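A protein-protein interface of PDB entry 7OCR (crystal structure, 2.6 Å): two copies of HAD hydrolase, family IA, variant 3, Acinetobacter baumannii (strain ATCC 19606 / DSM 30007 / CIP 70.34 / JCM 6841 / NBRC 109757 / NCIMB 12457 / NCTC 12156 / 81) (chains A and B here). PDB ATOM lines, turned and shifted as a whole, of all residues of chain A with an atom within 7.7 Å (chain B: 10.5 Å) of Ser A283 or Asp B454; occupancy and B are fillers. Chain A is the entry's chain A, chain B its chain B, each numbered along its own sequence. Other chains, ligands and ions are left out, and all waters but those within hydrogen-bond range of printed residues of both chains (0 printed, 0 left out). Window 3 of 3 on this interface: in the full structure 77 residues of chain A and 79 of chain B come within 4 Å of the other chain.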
ATOM      1  N   THR A 280      -2.108   9.451   9.724  1.00  0.00           N
ATOM      2  CA  THR A 280      -2.905  10.337   8.831  1.00  0.00           C
ATOM      3  C   THR A 280      -3.474  11.512   9.636  1.00  0.00           C
ATOM      4  O   THR A 280      -3.810  11.311  10.820  1.00  0.00           O
ATOM      5  CB  THR A 280      -4.018   9.553   8.121  1.00  0.00           C
ATOM      6  OG1 THR A 280      -4.637  10.420   7.171  1.00  0.00           O
ATOM      7  CG2 THR A 280      -5.064   9.006   9.068  1.00  0.00           C
ATOM      8  N   ARG A 281      -3.569  12.688   9.006  1.00  0.00           N
ATOM      9  CA  ARG A 281      -4.181  13.919   9.580  1.00  0.00           C
ATOM     10  C   ARG A 281      -5.693  13.898   9.323  1.00  0.00           C
ATOM     11  O   ARG A 281      -6.413  14.666   9.993  1.00  0.00           O
ATOM     12  CB  ARG A 281      -3.545  15.171   8.966  1.00  0.00           C
ATOM     13  CG  ARG A 281      -2.031  15.248   9.119  1.00  0.00           C
ATOM     14  CD  ARG A 281      -1.405  16.238   8.153  1.00  0.00           C
ATOM     15  NE  ARG A 281      -1.559  15.825   6.762  1.00  0.00           N
ATOM     16  CZ  ARG A 281      -1.257  16.573   5.701  1.00  0.00           C
ATOM     17  NH1 ARG A 281      -0.774  17.797   5.853  1.00  0.00           N
ATOM     18  NH2 ARG A 281      -1.442  16.092   4.483  1.00  0.00           N
ATOM     19  N   ASN A 282      -6.145  13.061   8.382  1.00  0.00           N
ATOM     20  CA  ASN A 282      -7.577  12.859   8.027  1.00  0.00           C
ATOM     21  C   ASN A 282      -8.282  12.167   9.202  1.00  0.00           C
ATOM     22  O   ASN A 282      -8.133  10.936   9.341  1.00  0.00           O
ATOM     23  CB  ASN A 282      -7.716  12.071   6.721  1.00  0.00           C
ATOM     24  CG  ASN A 282      -9.121  12.077   6.156  1.00  0.00           C
ATOM     25  OD1 ASN A 282     -10.099  12.123   6.899  1.00  0.00           O
ATOM     26  ND2 ASN A 282      -9.232  12.023   4.839  1.00  0.00           N
ATOM     27  N   SER A 283      -9.019  12.939  10.007  1.00  0.00           N
ATOM     28  CA  SER A 283      -9.729  12.481  11.232  1.00  0.00           C
ATOM     29  C   SER A 283     -10.859  11.510  10.870  1.00  0.00           C
ATOM     30  O   SER A 283     -11.069  10.545  11.632  1.00  0.00           O
ATOM     31  CB  SER A 283     -10.247  13.654  12.024  1.00  0.00           C
ATOM     32  OG  SER A 283     -11.011  14.522  11.199  1.00  0.00           O
ATOM     33  N   LEU A 284     -11.559  11.759   9.757  1.00  0.00           N
ATOM     34  CA  LEU A 284     -12.695  10.926   9.270  1.00  0.00           C
ATOM     35  C   LEU A 284     -12.189   9.509   8.976  1.00  0.00           C
ATOM     36  O   LEU A 284     -12.813   8.551   9.469  1.00  0.00           O
ATOM     37  CB  LEU A 284     -13.303  11.570   8.018  1.00  0.00           C
ATOM     38  CG  LEU A 284     -14.600  10.939   7.511  1.00  0.00           C
ATOM     39  CD1 LEU A 284     -15.719  11.096   8.529  1.00  0.00           C
ATOM     40  CD2 LEU A 284     -15.009  11.540   6.176  1.00  0.00           C
ATOM     41  N   PHE A 285     -11.099   9.394   8.211  1.00  0.00           N
ATOM     42  CA  PHE A 285     -10.423   8.116   7.858  1.00  0.00           C
ATOM     43  C   PHE A 285      -9.982   7.385   9.133  1.00  0.00           C
ATOM     44  O   PHE A 285     -10.179   6.158   9.212  1.00  0.00           O
ATOM     45  CB  PHE A 285      -9.229   8.363   6.930  1.00  0.00           C
ATOM     46  CG  PHE A 285      -9.533   8.220   5.460  1.00  0.00           C
ATOM     47  CD1 PHE A 285     -10.400   9.094   4.823  1.00  0.00           C
ATOM     48  CD2 PHE A 285      -8.950   7.209   4.710  1.00  0.00           C
ATOM     49  CE1 PHE A 285     -10.678   8.960   3.470  1.00  0.00           C
ATOM     50  CE2 PHE A 285      -9.230   7.075   3.359  1.00  0.00           C
ATOM     51  CZ  PHE A 285     -10.093   7.950   2.741  1.00  0.00           C
ATOM     52  N   ARG A 286      -9.407   8.119  10.092  1.00  0.00           N
ATOM     53  CA  ARG A 286      -8.858   7.571  11.364  1.00  0.00           C
ATOM     54  C   ARG A 286      -9.992   6.955  12.193  1.00  0.00           C
ATOM     55  O   ARG A 286      -9.901   5.754  12.511  1.00  0.00           O
ATOM     56  CB  ARG A 286      -8.130   8.663  12.156  1.00  0.00           C
ATOM     57  CG  ARG A 286      -7.605   8.208  13.510  1.00  0.00           C
ATOM     58  CD  ARG A 286      -6.587   9.157  14.115  1.00  0.00           C
ATOM     59  NE  ARG A 286      -7.137  10.484  14.372  1.00  0.00           N
ATOM     60  CZ  ARG A 286      -6.966  11.558  13.600  1.00  0.00           C
ATOM     61  NH1 ARG A 286      -6.250  11.495  12.487  1.00  0.00           N
ATOM     62  NH2 ARG A 286      -7.522  12.707  13.949  1.00  0.00           N
ATOM     63  N   GLU A 287     -11.016   7.752  12.516  1.00  0.00           N
ATOM     64  CA  GLU A 287     -12.134   7.367  13.421  1.00  0.00           C
ATOM     65  C   GLU A 287     -12.976   6.259  12.774  1.00  0.00           C
ATOM     66  O   GLU A 287     -13.415   5.356  13.513  1.00  0.00           O
ATOM     67  CB  GLU A 287     -12.995   8.587  13.758  1.00  0.00           C
ATOM     68  CG  GLU A 287     -12.269   9.645  14.577  1.00  0.00           C
ATOM     69  CD  GLU A 287     -11.923   9.251  16.004  1.00  0.00           C
ATOM     70  OE1 GLU A 287     -12.432   8.214  16.477  1.00  0.00           O
ATOM     71  OE2 GLU A 287     -11.145   9.987  16.642  1.00  0.00           O
ATOM     72  N   ALA A 288     -13.185   6.324  11.453  1.00  0.00           N
ATOM     73  CA  ALA A 288     -13.997   5.361  10.667  1.00  0.00           C
ATOM     74  C   ALA A 288     -13.367   3.963  10.731  1.00  0.00           C
ATOM     75  O   ALA A 288     -14.097   3.003  11.047  1.00  0.00           O
ATOM     76  CB  ALA A 288     -14.133   5.831   9.239  1.00  0.00           C
ATOM     77  N   VAL A 289     -12.067   3.859  10.434  1.00  0.00           N
ATOM     78  CA  VAL A 289     -11.301   2.576  10.408  1.00  0.00           C
ATOM     79  C   VAL A 289     -11.268   1.988  11.825  1.00  0.00           C
ATOM     80  O   VAL A 289     -11.437   0.761  11.955  1.00  0.00           O
ATOM     81  CB  VAL A 289      -9.878   2.767   9.846  1.00  0.00           C
ATOM     82  CG1 VAL A 289      -9.017   1.527  10.037  1.00  0.00           C
ATOM     83  CG2 VAL A 289      -9.898   3.179   8.381  1.00  0.00           C
ATOM     84  N   ASN A 290     -11.054   2.835  12.837  1.00  0.00           N
ATOM     85  CA  ASN A 290     -10.977   2.437  14.270  1.00  0.00           C
ATOM     86  C   ASN A 290     -12.360   1.985  14.756  1.00  0.00           C
ATOM     87  O   ASN A 290     -12.409   1.078  15.611  1.00  0.00           O
ATOM     88  CB  ASN A 290     -10.410   3.563  15.139  1.00  0.00           C
ATOM     89  CG  ASN A 290      -8.948   3.852  14.863  1.00  0.00           C
ATOM     90  OD1 ASN A 290      -8.311   3.171  14.062  1.00  0.00           O
ATOM     91  ND2 ASN A 290      -8.405   4.863  15.521  1.00  0.00           N
ATOM     92  N   ILE A 313      -5.195   3.150  13.239  1.00  0.00           N
ATOM     93  CA  ILE A 313      -4.916   4.474  12.606  1.00  0.00           C
ATOM     94  C   ILE A 313      -4.671   5.497  13.722  1.00  0.00           C
ATOM     95  O   ILE A 313      -5.449   5.502  14.697  1.00  0.00           O
ATOM     96  CB  ILE A 313      -6.055   4.912  11.660  1.00  0.00           C
ATOM     97  CG1 ILE A 313      -6.520   3.781  10.736  1.00  0.00           C
ATOM     98  CG2 ILE A 313      -5.646   6.146  10.868  1.00  0.00           C
ATOM     99  CD1 ILE A 313      -5.425   3.185   9.878  1.00  0.00           C
ATOM    100  N   ASP A 315      -3.040   9.766  14.721  1.00  0.00           N
ATOM    101  CA  ASP A 315      -2.836  11.170  14.274  1.00  0.00           C
ATOM    102  C   ASP A 315      -1.338  11.389  14.028  1.00  0.00           C
ATOM    103  O   ASP A 315      -0.537  11.017  14.908  1.00  0.00           O
ATOM    104  CB  ASP A 315      -3.387  12.160  15.305  1.00  0.00           C
ATOM    105  CG  ASP A 315      -3.536  13.587  14.799  1.00  0.00           C
ATOM    106  OD1 ASP A 315      -2.848  13.946  13.822  1.00  0.00           O
ATOM    107  OD2 ASP A 315      -4.343  14.331  15.390  1.00  0.00           O
ATOM    108  N   ASP A 317       0.160  14.241  13.922  1.00  0.00           N
ATOM    109  CA  ASP A 317       0.559  15.364  14.814  1.00  0.00           C
ATOM    110  C   ASP A 317       0.843  14.833  16.226  1.00  0.00           C
ATOM    111  O   ASP A 317       1.763  15.367  16.877  1.00  0.00           O
ATOM    112  CB  ASP A 317      -0.515  16.456  14.846  1.00  0.00           C
ATOM    113  CG  ASP A 317      -0.794  17.092  13.494  1.00  0.00           C
ATOM    114  OD1 ASP A 317       0.060  16.962  12.592  1.00  0.00           O
ATOM    115  OD2 ASP A 317      -1.865  17.715  13.353  1.00  0.00           O
ATOM    116  N   ASN A 423     -13.573  12.340   0.850  1.00  0.00           N
ATOM    117  CA  ASN A 423     -14.314  12.497   2.131  1.00  0.00           C
ATOM    118  C   ASN A 423     -15.814  12.625   1.836  1.00  0.00           C
ATOM    119  O   ASN A 423     -16.620  12.222   2.699  1.00  0.00           O
ATOM    120  CB  ASN A 423     -13.793  13.690   2.936  1.00  0.00           C
ATOM    121  CG  ASN A 423     -12.335  13.546   3.311  1.00  0.00           C
ATOM    122  OD1 ASN A 423     -11.940  12.548   3.910  1.00  0.00           O
ATOM    123  ND2 ASN A 423     -11.525  14.532   2.960  1.00  0.00           N
ATOM    124  N   LEU A 426     -16.809   9.017   1.186  1.00  0.00           N
ATOM    125  CA  LEU A 426     -16.675   8.294   2.480  1.00  0.00           C
ATOM    126  C   LEU A 426     -17.903   8.585   3.351  1.00  0.00           C
ATOM    127  O   LEU A 426     -18.488   7.621   3.878  1.00  0.00           O
ATOM    128  CB  LEU A 426     -15.380   8.719   3.180  1.00  0.00           C
ATOM    129  CG  LEU A 426     -15.113   8.064   4.536  1.00  0.00           C
ATOM    130  CD1 LEU A 426     -15.282   6.553   4.463  1.00  0.00           C
ATOM    131  CD2 LEU A 426     -13.723   8.417   5.042  1.00  0.00           C
ATOM    132  N   GLU B 453     -14.096  14.748  14.694  1.00  0.00           N
ATOM    133  CA  GLU B 453     -13.650  15.122  13.323  1.00  0.00           C
ATOM    134  C   GLU B 453     -13.300  16.616  13.296  1.00  0.00           C
ATOM    135  O   GLU B 453     -14.029  17.402  13.931  1.00  0.00           O
ATOM    136  CB  GLU B 453     -14.729  14.795  12.286  1.00  0.00           C
ATOM    137  CG  GLU B 453     -14.834  13.316  11.953  1.00  0.00           C
ATOM    138  CD  GLU B 453     -15.510  12.447  13.001  1.00  0.00           C
ATOM    139  OE1 GLU B 453     -15.905  12.984  14.056  1.00  0.00           O
ATOM    140  OE2 GLU B 453     -15.640  11.231  12.758  1.00  0.00           O
ATOM    141  N   ASP B 454     -12.234  16.980  12.575  1.00  0.00           N
ATOM    142  CA  ASP B 454     -11.668  18.357  12.530  1.00  0.00           C
ATOM    143  C   ASP B 454     -12.309  19.133  11.371  1.00  0.00           C
ATOM    144  O   ASP B 454     -13.287  19.861  11.627  1.00  0.00           O
ATOM    145  CB  ASP B 454     -10.139  18.317  12.442  1.00  0.00           C
ATOM    146  CG  ASP B 454      -9.463  17.746  13.678  1.00  0.00           C
ATOM    147  OD1 ASP B 454     -10.061  16.857  14.318  1.00  0.00           O
ATOM    148  OD2 ASP B 454      -8.342  18.195  13.991  1.00  0.00           O
ATOM    149  N   CYS B 455     -11.776  18.984  10.152  1.00  0.00           N
ATOM    150  CA  CYS B 455     -12.232  19.673   8.913  1.00  0.00           C
ATOM    151  C   CYS B 455     -11.575  19.013   7.693  1.00  0.00           C
ATOM    152  O   CYS B 455     -10.371  19.257   7.472  1.00  0.00           O
ATOM    153  CB  CYS B 455     -11.897  21.160   8.948  1.00  0.00           C
ATOM    154  SG  CYS B 455     -13.095  22.157   9.871  1.00  0.00           S
ATOM    155  N   ASN B 456     -12.341  18.215   6.940  1.00  0.00           N
ATOM    156  CA  ASN B 456     -11.838  17.359   5.830  1.00  0.00           C
ATOM    157  C   ASN B 456     -12.674  17.606   4.568  1.00  0.00           C
ATOM    158  O   ASN B 456     -13.239  16.631   4.031  1.00  0.00           O
ATOM    159  CB  ASN B 456     -11.834  15.882   6.237  1.00  0.00           C
ATOM    160  CG  ASN B 456     -10.984  15.610   7.460  1.00  0.00           C
ATOM    161  OD1 ASN B 456      -9.783  15.871   7.458  1.00  0.00           O
ATOM    162  ND2 ASN B 456     -11.596  15.086   8.510  1.00  0.00           N
ATOM    163  N   LYS B 457     -12.739  18.865   4.117  1.00  0.00           N
ATOM    164  CA  LYS B 457     -13.387  19.297   2.844  1.00  0.00           C
ATOM    165  C   LYS B 457     -14.885  18.957   2.874  1.00  0.00           C
ATOM    166  O   LYS B 457     -15.432  18.606   1.808  1.00  0.00           O
ATOM    167  CB  LYS B 457     -12.690  18.641   1.646  1.00  0.00           C
ATOM    168  CG  LYS B 457     -11.174  18.784   1.614  1.00  0.00           C
ATOM    169  CD  LYS B 457     -10.513  17.966   0.527  1.00  0.00           C
ATOM    170  CE  LYS B 457      -9.002  17.982   0.610  1.00  0.00           C
ATOM    171  NZ  LYS B 457      -8.388  17.090  -0.402  1.00  0.00           N
ATOM    172  N   LEU B 458     -15.517  19.069   4.048  1.00  0.00           N
ATOM    173  CA  LEU B 458     -16.969  18.823   4.268  1.00  0.00           C
ATOM    174  C   LEU B 458     -17.564  19.998   5.051  1.00  0.00           C
ATOM    175  O   LEU B 458     -16.788  20.738   5.688  1.00  0.00           O
ATOM    176  CB  LEU B 458     -17.148  17.507   5.035  1.00  0.00           C
ATOM    177  CG  LEU B 458     -16.765  16.237   4.278  1.00  0.00           C
ATOM    178  CD1 LEU B 458     -16.674  15.050   5.224  1.00  0.00           C
ATOM    179  CD2 LEU B 458     -17.749  15.950   3.154  1.00  0.00           C
ATOM    180  N   THR B 459     -18.891  20.154   5.005  1.00  0.00           N
ATOM    181  CA  THR B 459     -19.646  21.224   5.711  1.00  0.00           C
ATOM    182  C   THR B 459     -19.705  20.897   7.203  1.00  0.00           C
ATOM    183  O   THR B 459     -19.583  19.735   7.585  1.00  0.00           O
ATOM    184  CB  THR B 459     -21.050  21.400   5.118  1.00  0.00           C
ATOM    185  OG1 THR B 459     -21.745  20.158   5.226  1.00  0.00           O
ATOM    186  CG2 THR B 459     -21.025  21.844   3.671  1.00  0.00           C
ATOM    187  N   PRO B 460     -19.879  21.907   8.090  1.00  0.00           N
ATOM    188  CA  PRO B 460     -20.052  21.659   9.523  1.00  0.00           C
ATOM    189  C   PRO B 460     -21.241  20.741   9.856  1.00  0.00           C
ATOM    190  O   PRO B 460     -21.157  20.020  10.835  1.00  0.00           O
ATOM    191  CB  PRO B 460     -20.295  23.058  10.111  1.00  0.00           C
ATOM    192  CG  PRO B 460     -19.660  24.001   9.114  1.00  0.00           C
ATOM    193  CD  PRO B 460     -19.879  23.343   7.768  1.00  0.00           C
ATOM    194  N   ASP B 461     -22.306  20.797   9.048  1.00  0.00           N
ATOM    195  CA  ASP B 461     -23.535  19.971   9.198  1.00  0.00           C
ATOM    196  C   ASP B 461     -23.198  18.501   8.919  1.00  0.00           C
ATOM    197  O   ASP B 461     -23.578  17.644   9.743  1.00  0.00           O
ATOM    198  CB  ASP B 461     -24.653  20.461   8.272  1.00  0.00           C
ATOM    199  CG  ASP B 461     -25.132  21.872   8.572  1.00  0.00           C
ATOM    200  OD1 ASP B 461     -24.460  22.566   9.362  1.00  0.00           O
ATOM    201  OD2 ASP B 461     -26.174  22.266   8.010  1.00  0.00           O
ATOM    202  N   GLN B 462     -22.518  18.230   7.800  1.00  0.00           N
ATOM    203  CA  GLN B 462     -22.071  16.872   7.381  1.00  0.00           C
ATOM    204  C   GLN B 462     -21.084  16.312   8.413  1.00  0.00           C
ATOM    205  O   GLN B 462     -21.251  15.142   8.811  1.00  0.00           O
ATOM    206  CB  GLN B 462     -21.423  16.920   5.994  1.00  0.00           C
ATOM    207  CG  GLN B 462     -22.426  17.046   4.855  1.00  0.00           C
ATOM    208  CD  GLN B 462     -21.753  17.139   3.507  1.00  0.00           C
ATOM    209  OE1 GLN B 462     -20.690  17.735   3.359  1.00  0.00           O
ATOM    210  NE2 GLN B 462     -22.380  16.545   2.504  1.00  0.00           N
ATOM    211  N   LEU B 463     -20.099  17.122   8.818  1.00  0.00           N
ATOM    212  CA  LEU B 463     -19.042  16.754   9.801  1.00  0.00           C
ATOM    213  C   LEU B 463     -19.694  16.343  11.126  1.00  0.00           C
ATOM    214  O   LEU B 463     -19.292  15.302  11.682  1.00  0.00           O
ATOM    215  CB  LEU B 463     -18.102  17.948  10.004  1.00  0.00           C
ATOM    216  CG  LEU B 463     -16.798  17.636  10.738  1.00  0.00           C
ATOM    217  CD1 LEU B 463     -15.686  17.298   9.754  1.00  0.00           C
ATOM    218  CD2 LEU B 463     -16.383  18.798  11.627  1.00  0.00           C
ATOM    219  N   ASN B 464     -20.654  17.140  11.608  1.00  0.00           N
ATOM    220  CA  ASN B 464     -21.404  16.902  12.871  1.00  0.00           C
ATOM    221  C   ASN B 464     -22.244  15.626  12.733  1.00  0.00           C
ATOM    222  O   ASN B 464     -22.316  14.861  13.715  1.00  0.00           O
ATOM    223  CB  ASN B 464     -22.280  18.101  13.246  1.00  0.00           C
ATOM    224  CG  ASN B 464     -22.956  17.948  14.592  1.00  0.00           C
ATOM    225  OD1 ASN B 464     -22.376  17.402  15.527  1.00  0.00           O
ATOM    226  ND2 ASN B 464     -24.183  18.431  14.702  1.00  0.00           N
ATOM    227  N   ALA B 466     -21.615  13.117  10.557  1.00  0.00           N
ATOM    228  CA  ALA B 466     -20.607  12.041  10.395  1.00  0.00           C
ATOM    229  C   ALA B 466     -20.124  11.566  11.771  1.00  0.00           C
ATOM    230  O   ALA B 466     -19.970  10.342  11.951  1.00  0.00           O
ATOM    231  CB  ALA B 466     -19.456  12.532   9.550  1.00  0.00           C
ATOM    232  N   SER B 467     -19.889  12.503  12.696  1.00  0.00           N
ATOM    233  CA  SER B 467     -19.432  12.245  14.088  1.00  0.00           C
ATOM    234  C   SER B 467     -20.440  11.346  14.815  1.00  0.00           C
ATOM    235  O   SER B 467     -19.996  10.412  15.508  1.00  0.00           O
ATOM    236  CB  SER B 467     -19.212  13.534  14.837  1.00  0.00           C
ATOM    237  OG  SER B 467     -18.219  14.325  14.204  1.00  0.00           O
ATOM    238  N   VAL B 470     -20.331   7.639  13.256  1.00  0.00           N
ATOM    239  CA  VAL B 470     -19.065   6.941  13.639  1.00  0.00           C
ATOM    240  C   VAL B 470     -19.098   6.611  15.138  1.00  0.00           C
ATOM    241  O   VAL B 470     -18.578   5.541  15.510  1.00  0.00           O
ATOM    242  CB  VAL B 470     -17.827   7.780  13.264  1.00  0.00           C
ATOM    243  CG1 VAL B 470     -16.544   7.204  13.844  1.00  0.00           C
ATOM    244  CG2 VAL B 470     -17.696   7.947  11.757  1.00  0.00           C
ATOM    245  N   ASP B 471     -19.690   7.489  15.959  1.00  0.00           N
ATOM    246  CA  ASP B 471     -19.736   7.361  17.441  1.00  0.00           C
ATOM    247  C   ASP B 471     -20.526   6.105  17.831  1.00  0.00           C
ATOM    248  O   ASP B 471     -19.982   5.288  18.599  1.00  0.00           O
ATOM    249  CB  ASP B 471     -20.337   8.609  18.095  1.00  0.00           C
ATOM    250  CG  ASP B 471     -20.434   8.528  19.610  1.00  0.00           C
ATOM    251  OD1 ASP B 471     -21.441   9.020  20.159  1.00  0.00           O
ATOM    252  OD2 ASP B 471     -19.500   7.979  20.231  1.00  0.00           O
ATOM    253  N   ARG B 474     -18.958   2.821  16.345  1.00  0.00           N
ATOM    254  CA  ARG B 474     -17.876   2.382  17.270  1.00  0.00           C
ATOM    255  C   ARG B 474     -18.510   1.703  18.491  1.00  0.00           C
ATOM    256  O   ARG B 474     -18.063   0.599  18.847  1.00  0.00           O
ATOM    257  CB  ARG B 474     -17.008   3.570  17.705  1.00  0.00           C
ATOM    258  CG  ARG B 474     -15.715   3.172  18.405  1.00  0.00           C
ATOM    259  CD  ARG B 474     -14.966   4.346  19.008  1.00  0.00           C
ATOM    260  NE  ARG B 474     -15.490   4.723  20.317  1.00  0.00           N
ATOM    261  CZ  ARG B 474     -16.394   5.676  20.551  1.00  0.00           C
ATOM    262  NH1 ARG B 474     -16.785   5.914  21.793  1.00  0.00           N
ATOM    263  NH2 ARG B 474     -16.903   6.390  19.562  1.00  0.00           N
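No position is printed for both chains.
Of the 10 pairs that touch across the chains among the printed residues, none has its exchanged pair printed and touching as well.
The side-chain hydroxyl (OG1) of Thr A280 lies within hydrogen-bond range of the backbone NH (N) of Asn A282.
The side-chain amide nitrogen (ND2) of Asn A282 lies within hydrogen-bond range of the side-chain amide oxygen (OD1) of Asn A423 (2.9 Å).
The side-chain amide oxygen (OD1) of Asn A282 lies within hydrogen-bond range of the backbone NH (N) of Phe A285 (3.2 Å).
The side-chain carboxylate of Glu B453 lies within hydrogen-bond range of the side-chain hydroxyl of Ser B467 (2.7 Å).
OD1 of Asn A282 sits at hydrogen-bond distance from N of Leu A284, 3.2 Å away.
ND2 of Asn B456 sits at hydrogen-bond distance from OG of Ser A283 (2.8 Å).
The side-chain amide nitrogen of Asn A423 sits at hydrogen-bond distance from the backbone carbonyl oxygen of Asn B456, at 2.9 Å.
OG of Ser A283 is in hydrogen-bond range of N of Asp B454 (3.1 Å).
Asn A282 touches Asn B456 (OD1 to CG, 3.6 Å).
OG of Ser A283 touches CA of Glu B453, at 3.4 Å.
Asn B456 touches Leu A284.
CD2 of Leu A284 touches CD1 of Leu B458 (3.9998 Å).
Glu A287 touches Glu B453 (CB to OE2, 3.9 Å).
Glu A287 touches Val B470.
O of Asn A423 touches CD1 of Leu B458 (3.8 Å).
Of chain B, only Asn B456 comes within 4 Å of Asn A282.
Of the printed residues of chain B, Ser A283 touches Glu B453, Asp B454 and Asn B456.
Arg A286 touches none of the printed residues of chain B.
Of the printed residues of chain B, Asn A423 touches Asn B456 and Leu B458.
Printed residues of chain A within 4 Å of Glu B453: Ser A283 and Glu A287.
Of chain A, only Ser A283 comes within 4 Å of Asp B454.
Asn B464 touches none of the printed residues of chain A.
Of the 17 printed residues of chain B, 5 touch a printed residue of chain A.
Hydrophobic or aromatic side chains of chain A within 4 Å of the printed part of chain B: Leu A284.
Along chain A the printed residues that touch a printed residue of chain B span positions 282 to 423.
Among the printed residues, 10 pairs touch across the chains.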
